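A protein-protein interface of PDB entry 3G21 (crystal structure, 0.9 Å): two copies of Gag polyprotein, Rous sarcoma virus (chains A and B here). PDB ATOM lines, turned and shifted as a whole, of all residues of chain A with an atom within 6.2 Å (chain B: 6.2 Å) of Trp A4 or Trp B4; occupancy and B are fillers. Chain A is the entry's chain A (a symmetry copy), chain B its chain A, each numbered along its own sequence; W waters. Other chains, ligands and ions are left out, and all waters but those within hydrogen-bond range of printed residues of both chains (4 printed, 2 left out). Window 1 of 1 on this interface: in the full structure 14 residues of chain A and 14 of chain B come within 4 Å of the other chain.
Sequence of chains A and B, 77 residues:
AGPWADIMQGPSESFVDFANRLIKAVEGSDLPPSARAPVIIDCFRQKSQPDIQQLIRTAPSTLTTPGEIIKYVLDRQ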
ATOM      1  N   ALA A   1       3.763 -18.575  10.981  1.00  0.00           N
ATOM      2  CA  ALA A   1       4.407 -17.947   9.858  1.00  0.00           C
ATOM      3  C   ALA A   1       4.236 -18.816   8.619  1.00  0.00           C
ATOM      4  O   ALA A   1       3.808 -19.982   8.798  1.00  0.00           O
ATOM      5  CB  ALA A   1       5.867 -17.690  10.198  1.00  0.00           C
ATOM      6  N   GLY A   2       4.512 -18.285   7.427  1.00  0.00           N
ATOM      7  CA  GLY A   2       4.291 -19.009   6.208  1.00  0.00           C
ATOM      8  C   GLY A   2       5.294 -20.115   5.949  1.00  0.00           C
ATOM      9  O   GLY A   2       6.369 -20.135   6.566  1.00  0.00           O
ATOM     10  N   PRO A   3       4.969 -21.065   5.065  1.00  0.00           N
ATOM     11  CA  PRO A   3       5.945 -22.092   4.815  1.00  0.00           C
ATOM     12  C   PRO A   3       7.047 -21.564   3.937  1.00  0.00           C
ATOM     13  O   PRO A   3       6.916 -21.485   2.718  1.00  0.00           O
ATOM     14  CB  PRO A   3       5.229 -23.261   4.195  1.00  0.00           C
ATOM     15  CG  PRO A   3       3.972 -22.685   3.645  1.00  0.00           C
ATOM     16  CD  PRO A   3       3.757 -21.417   4.408  1.00  0.00           C
ATOM     17  N   TRP A   4       8.186 -21.202   4.586  1.00  0.00           N
ATOM     18  CA  TRP A   4       9.265 -20.552   3.872  1.00  0.00           C
ATOM     19  C   TRP A   4       9.784 -21.324   2.690  1.00  0.00           C
ATOM     20  O   TRP A   4      10.194 -20.745   1.711  1.00  0.00           O
ATOM     21  CB  TRP A   4      10.404 -20.134   4.825  1.00  0.00           C
ATOM     22  CG  TRP A   4      11.103 -21.269   5.436  1.00  0.00           C
ATOM     23  CD1 TRP A   4      10.867 -21.803   6.706  1.00  0.00           C
ATOM     24  CD2 TRP A   4      12.167 -22.053   4.884  1.00  0.00           C
ATOM     25  NE1 TRP A   4      11.708 -22.850   6.950  1.00  0.00           N
ATOM     26  CE2 TRP A   4      12.514 -23.023   5.831  1.00  0.00           C
ATOM     27  CE3 TRP A   4      12.841 -22.037   3.668  1.00  0.00           C
ATOM     28  CZ2 TRP A   4      13.496 -23.953   5.627  1.00  0.00           C
ATOM     29  CZ3 TRP A   4      13.828 -22.967   3.424  1.00  0.00           C
ATOM     30  CH2 TRP A   4      14.134 -23.913   4.413  1.00  0.00           C
ATOM     31  N   ALA A   5       9.794 -22.682   2.799  1.00  0.00           N
ATOM     32  CA  ALA A   5      10.362 -23.492   1.756  1.00  0.00           C
ATOM     33  C   ALA A   5       9.435 -23.594   0.538  1.00  0.00           C
ATOM     34  O   ALA A   5       9.902 -24.123  -0.512  1.00  0.00           O
ATOM     35  CB  ALA A   5      10.757 -24.855   2.299  1.00  0.00           C
ATOM     36  N   ASP A   6       8.226 -23.096   0.648  1.00  0.00           N
ATOM     37  CA  ASP A   6       7.266 -23.051  -0.462  1.00  0.00           C
ATOM     38  C   ASP A   6       7.224 -21.729  -1.178  1.00  0.00           C
ATOM     39  O   ASP A   6       6.566 -21.578  -2.180  1.00  0.00           O
ATOM     40  CB  ASP A   6       5.818 -23.160   0.082  1.00  0.00           C
ATOM     41  CG  ASP A   6       5.350 -24.439   0.566  1.00  0.00           C
ATOM     42  OD1 ASP A   6       6.023 -25.391   0.183  1.00  0.00           O
ATOM     43  OD2 ASP A   6       4.280 -24.434   1.215  1.00  0.00           O
ATOM     44  N   ILE A   7       7.950 -20.729  -0.718  1.00  0.00           N
ATOM     45  CA  ILE A   7       7.857 -19.393  -1.232  1.00  0.00           C
ATOM     46  C   ILE A   7       8.720 -19.193  -2.486  1.00  0.00           C
ATOM     47  O   ILE A   7       9.915 -19.517  -2.503  1.00  0.00           O
ATOM     48  CB  ILE A   7       8.240 -18.375  -0.169  1.00  0.00           C
ATOM     49  CG1 ILE A   7       7.154 -18.391   0.895  1.00  0.00           C
ATOM     50  CG2 ILE A   7       8.451 -16.920  -0.714  1.00  0.00           C
ATOM     51  CD1 ILE A   7       7.506 -17.546   2.061  1.00  0.00           C
ATOM     52  N   MET A   8       8.071 -18.775  -3.540  1.00  0.00           N
ATOM     53  CA  MET A   8       8.720 -18.547  -4.837  1.00  0.00           C
ATOM     54  C   MET A   8       8.245 -17.212  -5.365  1.00  0.00           C
ATOM     55  O   MET A   8       7.125 -16.803  -5.154  1.00  0.00           O
ATOM     56  CB  MET A   8       8.589 -19.678  -5.796  1.00  0.00           C
ATOM     57  CG  MET A   8       7.317 -19.766  -6.521  1.00  0.00           C
ATOM     58  SD  MET A   8       7.324 -21.340  -7.425  1.00  0.00           S
ATOM     59  CE  MET A   8       8.946 -21.441  -8.174  1.00  0.00           C
ATOM     60  N   LEU A  22       9.646 -13.987   1.893  1.00  0.00           N
ATOM     61  CA  LEU A  22      10.577 -15.055   2.259  1.00  0.00           C
ATOM     62  C   LEU A  22      11.205 -14.816   3.615  1.00  0.00           C
ATOM     63  O   LEU A  22      11.231 -15.705   4.480  1.00  0.00           O
ATOM     64  CB  LEU A  22      11.657 -15.195   1.191  1.00  0.00           C
ATOM     65  CG  LEU A  22      12.778 -16.198   1.491  1.00  0.00           C
ATOM     66  CD1 LEU A  22      12.267 -17.638   1.463  1.00  0.00           C
ATOM     67  CD2 LEU A  22      13.934 -15.961   0.565  1.00  0.00           C
ATOM     68  N   ALA A  25       8.878 -15.181   6.544  1.00  0.00           N
ATOM     69  CA  ALA A  25       8.598 -16.581   6.820  1.00  0.00           C
ATOM     70  C   ALA A  25       9.795 -17.281   7.479  1.00  0.00           C
ATOM     71  O   ALA A  25       9.621 -18.086   8.389  1.00  0.00           O
ATOM     72  CB  ALA A  25       8.177 -17.283   5.543  1.00  0.00           C
ATOM     73  N   VAL A  26      11.006 -17.002   7.021  1.00  0.00           N
ATOM     74  CA  VAL A  26      12.195 -17.582   7.646  1.00  0.00           C
ATOM     75  C   VAL A  26      12.322 -17.122   9.086  1.00  0.00           C
ATOM     76  O   VAL A  26      12.613 -17.898  10.004  1.00  0.00           O
ATOM     77  CB  VAL A  26      13.453 -17.281   6.812  1.00  0.00           C
ATOM     78  CG1 VAL A  26      14.712 -17.607   7.583  1.00  0.00           C
ATOM     79  CG2 VAL A  26      13.415 -18.022   5.482  1.00  0.00           C
ATOM     80  N   SER A  29      10.079 -19.015  11.430  1.00  0.00           N
ATOM     81  CA  SER A  29      10.306 -20.449  11.437  1.00  0.00           C
ATOM     82  C   SER A  29      11.028 -20.898  12.719  1.00  0.00           C
ATOM     83  O   SER A  29      11.483 -20.083  13.482  1.00  0.00           O
ATOM     84  CB  SER A  29      11.143 -20.856  10.225  1.00  0.00           C
ATOM     85  OG  SER A  29      12.458 -20.565  10.421  1.00  0.00           O
ATOM     86  N   ASP A  30      11.158 -22.205  12.820  1.00  0.00           N
ATOM     87  CA  ASP A  30      11.944 -22.813  13.896  1.00  0.00           C
ATOM     88  C   ASP A  30      13.409 -22.960  13.536  1.00  0.00           C
ATOM     89  O   ASP A  30      14.150 -23.633  14.317  1.00  0.00           O
ATOM     90  CB  ASP A  30      11.341 -24.143  14.366  1.00  0.00           C
ATOM     91  CG  ASP A  30      11.490 -25.217  13.349  1.00  0.00           C
ATOM     92  OD1 ASP A  30      11.926 -24.946  12.193  1.00  0.00           O
ATOM     93  OD2 ASP A  30      11.180 -26.368  13.670  1.00  0.00           O
ATOM     94  N   LEU A  31      14.008 -22.457  12.506  1.00  0.00           N
ATOM     95  CA  LEU A  31      15.361 -22.557  12.144  1.00  0.00           C
ATOM     96  C   LEU A  31      16.181 -21.871  13.253  1.00  0.00           C
ATOM     97  O   LEU A  31      15.756 -20.854  13.795  1.00  0.00           O
ATOM     98  CB  LEU A  31      15.636 -21.895  10.826  1.00  0.00           C
ATOM     99  CG  LEU A  31      15.009 -22.589   9.609  1.00  0.00           C
ATOM    100  CD1 LEU A  31      15.239 -21.721   8.373  1.00  0.00           C
ATOM    101  CD2 LEU A  31      15.622 -23.974   9.425  1.00  0.00           C
ATOM    102  N   PRO A  38      22.005 -17.992   5.610  1.00  0.00           N
ATOM    103  CA  PRO A  38      22.358 -18.883   4.506  1.00  0.00           C
ATOM    104  C   PRO A  38      21.138 -19.471   3.805  1.00  0.00           C
ATOM    105  O   PRO A  38      21.167 -19.668   2.591  1.00  0.00           O
ATOM    106  CB  PRO A  38      23.255 -19.938   5.168  1.00  0.00           C
ATOM    107  CG  PRO A  38      23.268 -19.672   6.562  1.00  0.00           C
ATOM    108  CD  PRO A  38      22.665 -18.356   6.868  1.00  0.00           C
ATOM    109  N   VAL A  39      20.078 -19.751   4.547  1.00  0.00           N
ATOM    110  CA  VAL A  39      18.822 -20.221   3.935  1.00  0.00           C
ATOM    111  C   VAL A  39      18.249 -19.164   3.023  1.00  0.00           C
ATOM    112  O   VAL A  39      17.825 -19.455   1.891  1.00  0.00           O
ATOM    113  CB  VAL A  39      17.850 -20.693   5.016  1.00  0.00           C
ATOM    114  CG1 VAL A  39      16.417 -20.798   4.459  1.00  0.00           C
ATOM    115  CG2 VAL A  39      18.306 -22.024   5.602  1.00  0.00           C
ATOM    116  N   ASP A  42      20.301 -18.952  -0.152  1.00  0.00           N
ATOM    117  CA  ASP A  42      20.019 -20.074  -1.074  1.00  0.00           C
ATOM    118  C   ASP A  42      18.659 -19.933  -1.750  1.00  0.00           C
ATOM    119  O   ASP A  42      18.501 -20.199  -2.922  1.00  0.00           O
ATOM    120  CB  ASP A  42      20.106 -21.420  -0.349  1.00  0.00           C
ATOM    121  CG  ASP A  42      21.466 -22.010  -0.114  1.00  0.00           C
ATOM    122  OD1 ASP A  42      22.480 -21.230  -0.228  1.00  0.00           O
ATOM    123  OD2 ASP A  42      21.646 -23.196   0.101  1.00  0.00           O
ATOM    124  N   CYS A  43      17.656 -19.507  -0.980  1.00  0.00           N
ATOM    125  CA  CYS A  43      16.335 -19.342  -1.562  1.00  0.00           C
ATOM    126  C   CYS A  43      16.284 -18.164  -2.542  1.00  0.00           C
ATOM    127  O   CYS A  43      15.566 -18.230  -3.545  1.00  0.00           O
ATOM    128  CB  CYS A  43      15.258 -19.161  -0.465  1.00  0.00           C
ATOM    129  SG  CYS A  43      14.968 -20.714   0.463  1.00  0.00           S
ATOM    130  N   GLN A  46      17.599 -19.801  -5.688  1.00  0.00           N
ATOM    131  CA  GLN A  46      16.864 -20.925  -6.229  1.00  0.00           C
ATOM    132  C   GLN A  46      15.388 -20.608  -6.563  1.00  0.00           C
ATOM    133  O   GLN A  46      14.792 -21.316  -7.346  1.00  0.00           O
ATOM    134  CB  GLN A  46      16.903 -22.085  -5.247  1.00  0.00           C
ATOM    135  CG  GLN A  46      18.293 -22.664  -5.045  1.00  0.00           C
ATOM    136  CD  GLN A  46      18.322 -23.727  -3.997  1.00  0.00           C
ATOM    137  OE1 GLN A  46      17.365 -24.489  -3.845  1.00  0.00           O
ATOM    138  NE2 GLN A  46      19.416 -23.840  -3.240  1.00  0.00           N
ATOM    139  N   LYS A  47      14.813 -19.620  -5.864  1.00  0.00           N
ATOM    140  CA  LYS A  47      13.368 -19.459  -5.855  1.00  0.00           C
ATOM    141  C   LYS A  47      12.902 -18.140  -6.488  1.00  0.00           C
ATOM    142  O   LYS A  47      11.702 -17.886  -6.577  1.00  0.00           O
ATOM    143  CB  LYS A  47      12.825 -19.588  -4.435  1.00  0.00           C
ATOM    144  CG  LYS A  47      13.247 -20.890  -3.726  1.00  0.00           C
ATOM    145  CD  LYS A  47      12.814 -22.149  -4.363  1.00  0.00           C
ATOM    146  CE  LYS A  47      11.340 -22.462  -4.170  1.00  0.00           C
ATOM    147  NZ  LYS A  47      11.070 -22.925  -2.801  1.00  0.00           N
ATOM    148  N   ALA B   1      25.125 -29.935  -6.972  1.00  0.00           N
ATOM    149  CA  ALA B   1      24.031 -30.627  -6.344  1.00  0.00           C
ATOM    150  C   ALA B   1      22.716 -29.970  -6.740  1.00  0.00           C
ATOM    151  O   ALA B   1      22.787 -28.854  -7.311  1.00  0.00           O
ATOM    152  CB  ALA B   1      24.248 -30.645  -4.839  1.00  0.00           C
ATOM    153  N   GLY B   2      21.578 -30.624  -6.495  1.00  0.00           N
ATOM    154  CA  GLY B   2      20.307 -30.112  -6.917  1.00  0.00           C
ATOM    155  C   GLY B   2      19.807 -28.935  -6.106  1.00  0.00           C
ATOM    156  O   GLY B   2      20.302 -28.691  -4.996  1.00  0.00           O
ATOM    157  N   PRO B   3      18.847 -28.168  -6.634  1.00  0.00           N
ATOM    158  CA  PRO B   3      18.369 -27.070  -5.837  1.00  0.00           C
ATOM    159  C   PRO B   3      17.456 -27.571  -4.751  1.00  0.00           C
ATOM    160  O   PRO B   3      16.277 -27.836  -4.972  1.00  0.00           O
ATOM    161  CB  PRO B   3      17.681 -26.100  -6.760  1.00  0.00           C
ATOM    162  CG  PRO B   3      17.342 -26.904  -7.966  1.00  0.00           C
ATOM    163  CD  PRO B   3      18.279 -28.068  -7.935  1.00  0.00           C
ATOM    164  N   TRP B   4      18.026 -27.689  -3.521  1.00  0.00           N
ATOM    165  CA  TRP B   4      17.293 -28.290  -2.426  1.00  0.00           C
ATOM    166  C   TRP B   4      15.975 -27.632  -2.122  1.00  0.00           C
ATOM    167  O   TRP B   4      15.041 -28.285  -1.721  1.00  0.00           O
ATOM    168  CB  TRP B   4      18.169 -28.421  -1.163  1.00  0.00           C
ATOM    169  CG  TRP B   4      18.554 -27.132  -0.581  1.00  0.00           C
ATOM    170  CD1 TRP B   4      19.763 -26.459  -0.781  1.00  0.00           C
ATOM    171  CD2 TRP B   4      17.800 -26.304   0.312  1.00  0.00           C
ATOM    172  NE1 TRP B   4      19.784 -25.289  -0.078  1.00  0.00           N
ATOM    173  CE2 TRP B   4      18.575 -25.174   0.598  1.00  0.00           C
ATOM    174  CE3 TRP B   4      16.533 -26.404   0.876  1.00  0.00           C
ATOM    175  CZ2 TRP B   4      18.154 -24.165   1.419  1.00  0.00           C
ATOM    176  CZ3 TRP B   4      16.073 -25.399   1.698  1.00  0.00           C
ATOM    177  CH2 TRP B   4      16.895 -24.293   1.951  1.00  0.00           C
ATOM    178  N   ALA B   5      15.908 -26.281  -2.295  1.00  0.00           N
ATOM    179  CA  ALA B   5      14.717 -25.560  -1.936  1.00  0.00           C
ATOM    180  C   ALA B   5      13.599 -25.750  -2.968  1.00  0.00           C
ATOM    181  O   ALA B   5      12.446 -25.318  -2.672  1.00  0.00           O
ATOM    182  CB  ALA B   5      15.038 -24.095  -1.692  1.00  0.00           C
ATOM    183  N   ASP B   6      13.894 -26.377  -4.082  1.00  0.00           N
ATOM    184  CA  ASP B   6      12.905 -26.700  -5.117  1.00  0.00           C
ATOM    185  C   ASP B   6      12.372 -28.104  -5.033  1.00  0.00           C
ATOM    186  O   ASP B   6      11.470 -28.477  -5.747  1.00  0.00           O
ATOM    187  CB  ASP B   6      13.576 -26.701  -6.514  1.00  0.00           C
ATOM    188  CG  ASP B   6      13.938 -25.438  -7.114  1.00  0.00           C
ATOM    189  OD1 ASP B   6      13.370 -24.471  -6.616  1.00  0.00           O
ATOM    190  OD2 ASP B   6      14.690 -25.488  -8.114  1.00  0.00           O
ATOM    191  N   ILE B   7      12.878 -28.929  -4.138  1.00  0.00           N
ATOM    192  CA  ILE B   7      12.551 -30.324  -4.086  1.00  0.00           C
ATOM    193  C   ILE B   7      11.251 -30.587  -3.313  1.00  0.00           C
ATOM    194  O   ILE B   7      11.069 -30.119  -2.181  1.00  0.00           O
ATOM    195  CB  ILE B   7      13.690 -31.125  -3.474  1.00  0.00           C
ATOM    196  CG1 ILE B   7      14.849 -31.100  -4.457  1.00  0.00           C
ATOM    197  CG2 ILE B   7      13.317 -32.604  -3.108  1.00  0.00           C
ATOM    198  CD1 ILE B   7      16.072 -31.720  -3.893  1.00  0.00           C
ATOM    199  N   MET B   8      10.332 -31.228  -3.984  1.00  0.00           N
ATOM    200  CA  MET B   8       9.014 -31.551  -3.421  1.00  0.00           C
ATOM    201  C   MET B   8       8.712 -32.997  -3.748  1.00  0.00           C
ATOM    202  O   MET B   8       9.088 -33.512  -4.776  1.00  0.00           O
ATOM    203  CB  MET B   8       7.937 -30.592  -3.791  1.00  0.00           C
ATOM    204  CG  MET B   8       7.342 -30.770  -5.120  1.00  0.00           C
ATOM    205  SD  MET B   8       6.248 -29.350  -5.410  1.00  0.00           S
ATOM    206  CE  MET B   8       5.330 -29.149  -3.888  1.00  0.00           C
ATOM    207  N   LEU B  22      16.139 -34.965  -1.297  1.00  0.00           N
ATOM    208  CA  LEU B  22      16.268 -33.746  -0.497  1.00  0.00           C
ATOM    209  C   LEU B  22      17.572 -33.710   0.271  1.00  0.00           C
ATOM    210  O   LEU B  22      18.309 -32.713   0.246  1.00  0.00           O
ATOM    211  CB  LEU B  22      15.085 -33.620   0.458  1.00  0.00           C
ATOM    212  CG  LEU B  22      15.138 -32.451   1.448  1.00  0.00           C
ATOM    213  CD1 LEU B  22      14.979 -31.106   0.740  1.00  0.00           C
ATOM    214  CD2 LEU B  22      14.136 -32.666   2.543  1.00  0.00           C
ATOM    215  N   ALA B  25      20.655 -33.237  -1.827  1.00  0.00           N
ATOM    216  CA  ALA B  25      20.776 -31.860  -2.276  1.00  0.00           C
ATOM    217  C   ALA B  25      21.214 -30.927  -1.137  1.00  0.00           C
ATOM    218  O   ALA B  25      22.027 -30.032  -1.345  1.00  0.00           O
ATOM    219  CB  ALA B  25      19.471 -31.404  -2.899  1.00  0.00           C
ATOM    220  N   VAL B  26      20.673 -31.111   0.057  1.00  0.00           N
ATOM    221  CA  VAL B  26      21.093 -30.303   1.201  1.00  0.00           C
ATOM    222  C   VAL B  26      22.559 -30.536   1.514  1.00  0.00           C
ATOM    223  O   VAL B  26      23.335 -29.607   1.769  1.00  0.00           O
ATOM    224  CB  VAL B  26      20.179 -30.554   2.414  1.00  0.00           C
ATOM    225  CG1 VAL B  26      20.768 -29.965   3.676  1.00  0.00           C
ATOM    226  CG2 VAL B  26      18.776 -30.018   2.159  1.00  0.00           C
ATOM    227  N   SER B  29      24.860 -28.634  -0.766  1.00  0.00           N
ATOM    228  CA  SER B  29      24.661 -27.196  -0.742  1.00  0.00           C
ATOM    229  C   SER B  29      25.794 -26.483   0.016  1.00  0.00           C
ATOM    230  O   SER B  29      26.604 -27.118   0.643  1.00  0.00           O
ATOM    231  CB  SER B  29      23.328 -26.860  -0.077  1.00  0.00           C
ATOM    232  OG  SER B  29      23.423 -26.950   1.278  1.00  0.00           O
ATOM    233  N   ASP B  30      25.714 -25.169  -0.031  1.00  0.00           N
ATOM    234  CA  ASP B  30      26.617 -24.321   0.750  1.00  0.00           C
ATOM    235  C   ASP B  30      26.091 -24.040   2.144  1.00  0.00           C
ATOM    236  O   ASP B  30      26.700 -23.175   2.847  1.00  0.00           O
ATOM    237  CB  ASP B  30      26.972 -23.026   0.008  1.00  0.00           C
ATOM    238  CG  ASP B  30      25.817 -22.095  -0.081  1.00  0.00           C
ATOM    239  OD1 ASP B  30      24.666 -22.468   0.289  1.00  0.00           O
ATOM    240  OD2 ASP B  30      26.018 -20.960  -0.521  1.00  0.00           O
ATOM    241  N   LEU B  31      25.078 -24.602   2.718  1.00  0.00           N
ATOM    242  CA  LEU B  31      24.569 -24.382   4.008  1.00  0.00           C
ATOM    243  C   LEU B  31      25.666 -24.795   5.007  1.00  0.00           C
ATOM    244  O   LEU B  31      26.374 -25.771   4.777  1.00  0.00           O
ATOM    245  CB  LEU B  31      23.325 -25.182   4.260  1.00  0.00           C
ATOM    246  CG  LEU B  31      22.100 -24.751   3.441  1.00  0.00           C
ATOM    247  CD1 LEU B  31      20.968 -25.747   3.685  1.00  0.00           C
ATOM    248  CD2 LEU B  31      21.678 -23.339   3.836  1.00  0.00           C
ATOM    249  N   PRO B  38      18.021 -28.933  10.649  1.00  0.00           N
ATOM    250  CA  PRO B  38      16.782 -28.168  10.777  1.00  0.00           C
ATOM    251  C   PRO B  38      16.141 -27.845   9.432  1.00  0.00           C
ATOM    252  O   PRO B  38      14.916 -27.818   9.330  1.00  0.00           O
ATOM    253  CB  PRO B  38      17.208 -26.925  11.570  1.00  0.00           C
ATOM    254  CG  PRO B  38      18.616 -26.988  11.739  1.00  0.00           C
ATOM    255  CD  PRO B  38      19.147 -28.315  11.356  1.00  0.00           C
ATOM    256  N   VAL B  39      16.947 -27.601   8.410  1.00  0.00           N
ATOM    257  CA  VAL B  39      16.412 -27.386   7.053  1.00  0.00           C
ATOM    258  C   VAL B  39      15.707 -28.625   6.559  1.00  0.00           C
ATOM    259  O   VAL B  39      14.596 -28.553   6.004  1.00  0.00           O
ATOM    260  CB  VAL B  39      17.518 -26.895   6.120  1.00  0.00           C
ATOM    261  CG1 VAL B  39      17.104 -27.053   4.645  1.00  0.00           C
ATOM    262  CG2 VAL B  39      17.880 -25.448   6.433  1.00  0.00           C
ATOM    263  N   ASP B  42      12.391 -29.017   8.344  1.00  0.00           N
ATOM    264  CA  ASP B  42      11.367 -28.080   7.830  1.00  0.00           C
ATOM    265  C   ASP B  42      10.858 -28.488   6.451  1.00  0.00           C
ATOM    266  O   ASP B  42       9.684 -28.411   6.158  1.00  0.00           O
ATOM    267  CB  ASP B  42      11.901 -26.646   7.788  1.00  0.00           C
ATOM    268  CG  ASP B  42      11.917 -25.860   9.066  1.00  0.00           C
ATOM    269  OD1 ASP B  42      11.800 -26.513  10.167  1.00  0.00           O
ATOM    270  OD2 ASP B  42      11.959 -24.643   9.096  1.00  0.00           O
ATOM    271  N   CYS B  43      11.776 -28.926   5.586  1.00  0.00           N
ATOM    272  CA  CYS B  43      11.358 -29.338   4.257  1.00  0.00           C
ATOM    273  C   CYS B  43      10.547 -30.639   4.289  1.00  0.00           C
ATOM    274  O   CYS B  43       9.624 -30.807   3.486  1.00  0.00           O
ATOM    275  CB  CYS B  43      12.575 -29.499   3.313  1.00  0.00           C
ATOM    276  SG  CYS B  43      13.322 -27.882   2.887  1.00  0.00           S
ATOM    277  N   GLN B  46       7.099 -29.306   5.089  1.00  0.00           N
ATOM    278  CA  GLN B  46       6.498 -28.372   4.160  1.00  0.00           C
ATOM    279  C   GLN B  46       6.361 -28.918   2.721  1.00  0.00           C
ATOM    280  O   GLN B  46       5.559 -28.409   1.966  1.00  0.00           O
ATOM    281  CB  GLN B  46       7.314 -27.090   4.120  1.00  0.00           C
ATOM    282  CG  GLN B  46       7.296 -26.316   5.426  1.00  0.00           C
ATOM    283  CD  GLN B  46       8.191 -25.121   5.394  1.00  0.00           C
ATOM    284  OE1 GLN B  46       8.343 -24.474   4.356  1.00  0.00           O
ATOM    285  NE2 GLN B  46       8.811 -24.764   6.522  1.00  0.00           N
ATOM    286  N   LYS B  47       7.236 -29.864   2.351  1.00  0.00           N
ATOM    287  CA  LYS B  47       7.414 -30.205   0.949  1.00  0.00           C
ATOM    288  C   LYS B  47       7.007 -31.649   0.621  1.00  0.00           C
ATOM    289  O   LYS B  47       7.075 -32.064  -0.534  1.00  0.00           O
ATOM    290  CB  LYS B  47       8.854 -29.949   0.516  1.00  0.00           C
ATOM    291  CG  LYS B  47       9.345 -28.516   0.810  1.00  0.00           C
ATOM    292  CD  LYS B  47       8.600 -27.425   0.152  1.00  0.00           C
ATOM    293  CE  LYS B  47       8.902 -27.279  -1.330  1.00  0.00           C
ATOM    294  NZ  LYS B  47      10.221 -26.667  -1.545  1.00  0.00           N
HETATM  295  O   HOH W   1       3.776 -26.558   2.561  1.00  0.00           O
HETATM  296  O   HOH W   2      15.798 -23.278  -8.795  1.00  0.00           O
HETATM  297  O   HOH W   3      23.973 -24.180  -2.223  1.00  0.00           O
HETATM  298  O   HOH W   4       9.302 -23.706  11.056  1.00  0.00           O
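Hydrophobic or aromatic side chains of chain B that line the printed part of chain A: Pro B3, Trp B4, Ala B5, Leu B31, Pro B38 and Val B39. Of the 20 printed residues of chain A, 11 touch a printed residue of chain B. Among the printed residues, 25 pairs touch across the chains. Among the printed residues, no Asp or Glu carboxylate lies within 4 Å of a Lys or Arg side-chain nitrogen of the other chain.
The backbone carbonyl oxygen (O) of Val A39 sits at hydrogen-bond distance from the side-chain sulfur (SG) of Cys A43, 3.4 Å away. SG of Cys B43 is in hydrogen-bond range of O of Val B39 (3.4 Å). The side-chain hydroxyl of Ser B29 is in hydrogen-bond range of the backbone NH of Leu B31 (3.2 Å). The backbone carbonyl oxygen (O) of Ala A5 lies within hydrogen-bond range of the side-chain amino group (NZ) of Lys A47, at 2.8 Å. OG of Ser A29 sits at hydrogen-bond distance from N of Leu A31 (3.2 Å).
Trp B4 touches its own counterpart, Trp A4. Trp A4 touches Gln B46, and with the chains exchanged Gln A46 touches Trp B4. Asp A6 touches Lys B47, and with the chains exchanged Lys A47 touches Asp B6. Leu A31 touches Val B39, and with the chains exchanged Val A39 touches Leu B31. Positions printed for both chains: 1, 2, 3, 4, 5, 6, 7, 8, 22, 25, 26, 29, 30, 31, 38, 39, 42, 43, 46 and 47.
Water W2 lies within hydrogen-bond range of the side-chain carboxylate (OD2) of Asp B6 (2.6 Å) and the backbone carbonyl oxygen (O) of Gln A46 (2.6 Å). Water W1 bridges OD2 of Asp A6 and O of Gln B46. Water W4 bridges N of Asp A30 (3.0 Å) and OD2 of Asp B42 (3.4 Å). Water W3 lies within hydrogen-bond range of the backbone NH of Asp B30 (3.0 Å) and the side-chain carboxylate of Asp A42 (3.4 Å).
Of the printed residues of chain B, Pro A3 touches Gln B46. Of chain B, only Trp B4 (3.7 Å), Asp B42 (2.8 Å) and Gln B46 (3.3 Å) come within 4 Å of Trp A4. Printed residues of chain B within 4 Å of Ala A5: Ala B5, Gln B46 and Lys B47. Val A26 touches none of the printed residues of chain B. Of the printed residues of chain A, Pro B3 touches Gln A46. Trp B4 touches just these residues of chain A: Trp A4 (3.7 Å), Asp A42 (2.8 Å) and Gln A46 (3.3 Å). Ser B29 touches none of the printed residues of chain A. Printed residues of chain A within 4 Å of Lys B47: Ala A5 and Asp A6. The nearest printed residue of chain A that does not touch Trp B4 is Val A39 (4.3 Å).
Gln B46 touches Pro A3 (OE1 to C, 3.2 Å). Trp B4 touches Trp A4. Ala A5 touches Ala B5. Asp A6 touches Gln B46. Leu A31 touches Pro B38. Val B39 touches Leu A31. OD2 of Asp B42 touches CG of Leu A31 (3.7 Å). Leu B31 touches Val A39 (CD2 to N, 3.99 Å). Leu B31 touches Asp A42 (CG to OD2, 3.7 Å). Asp B6 touches Lys A47.
The side-chain carboxylate (OD2) of Asp B42 sits at hydrogen-bond distance from the indole nitrogen (NE1) of Trp A4. NZ of Lys B47 is in hydrogen-bond range of O of Ala A5 (2.8 Å). The side-chain carboxylate (OD1) of Asp B42 sits close to the side-chain carboxylate (OD1) of Asp A30. The indole nitrogen (NE1) of Trp B4 lies within hydrogen-bond range of the side-chain carboxylate (OD2) of Asp A42, at 2.8 Å. The backbone NH (N) of Ala B5 sits at hydrogen-bond distance from the side-chain amide oxygen (OE1) of Gln A46. The side-chain amide oxygen (OE1) of Gln B46 is in hydrogen-bond range of the backbone NH (N) of Ala A5, at 2.8 Å. NZ of Lys A47 sits at hydrogen-bond distance from O of Ala B5, 2.8 Å away. The backbone NH of Trp B4 sits at hydrogen-bond distance from the side-chain amide oxygen of Gln A46 (3.3 Å). OD1 of Asp B30 sits close to OD1 of Asp A42 (2.6 Å). The backbone NH (N) of Trp A4 lies within hydrogen-bond range of the side-chain amide oxygen (OE1) of Gln B46.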
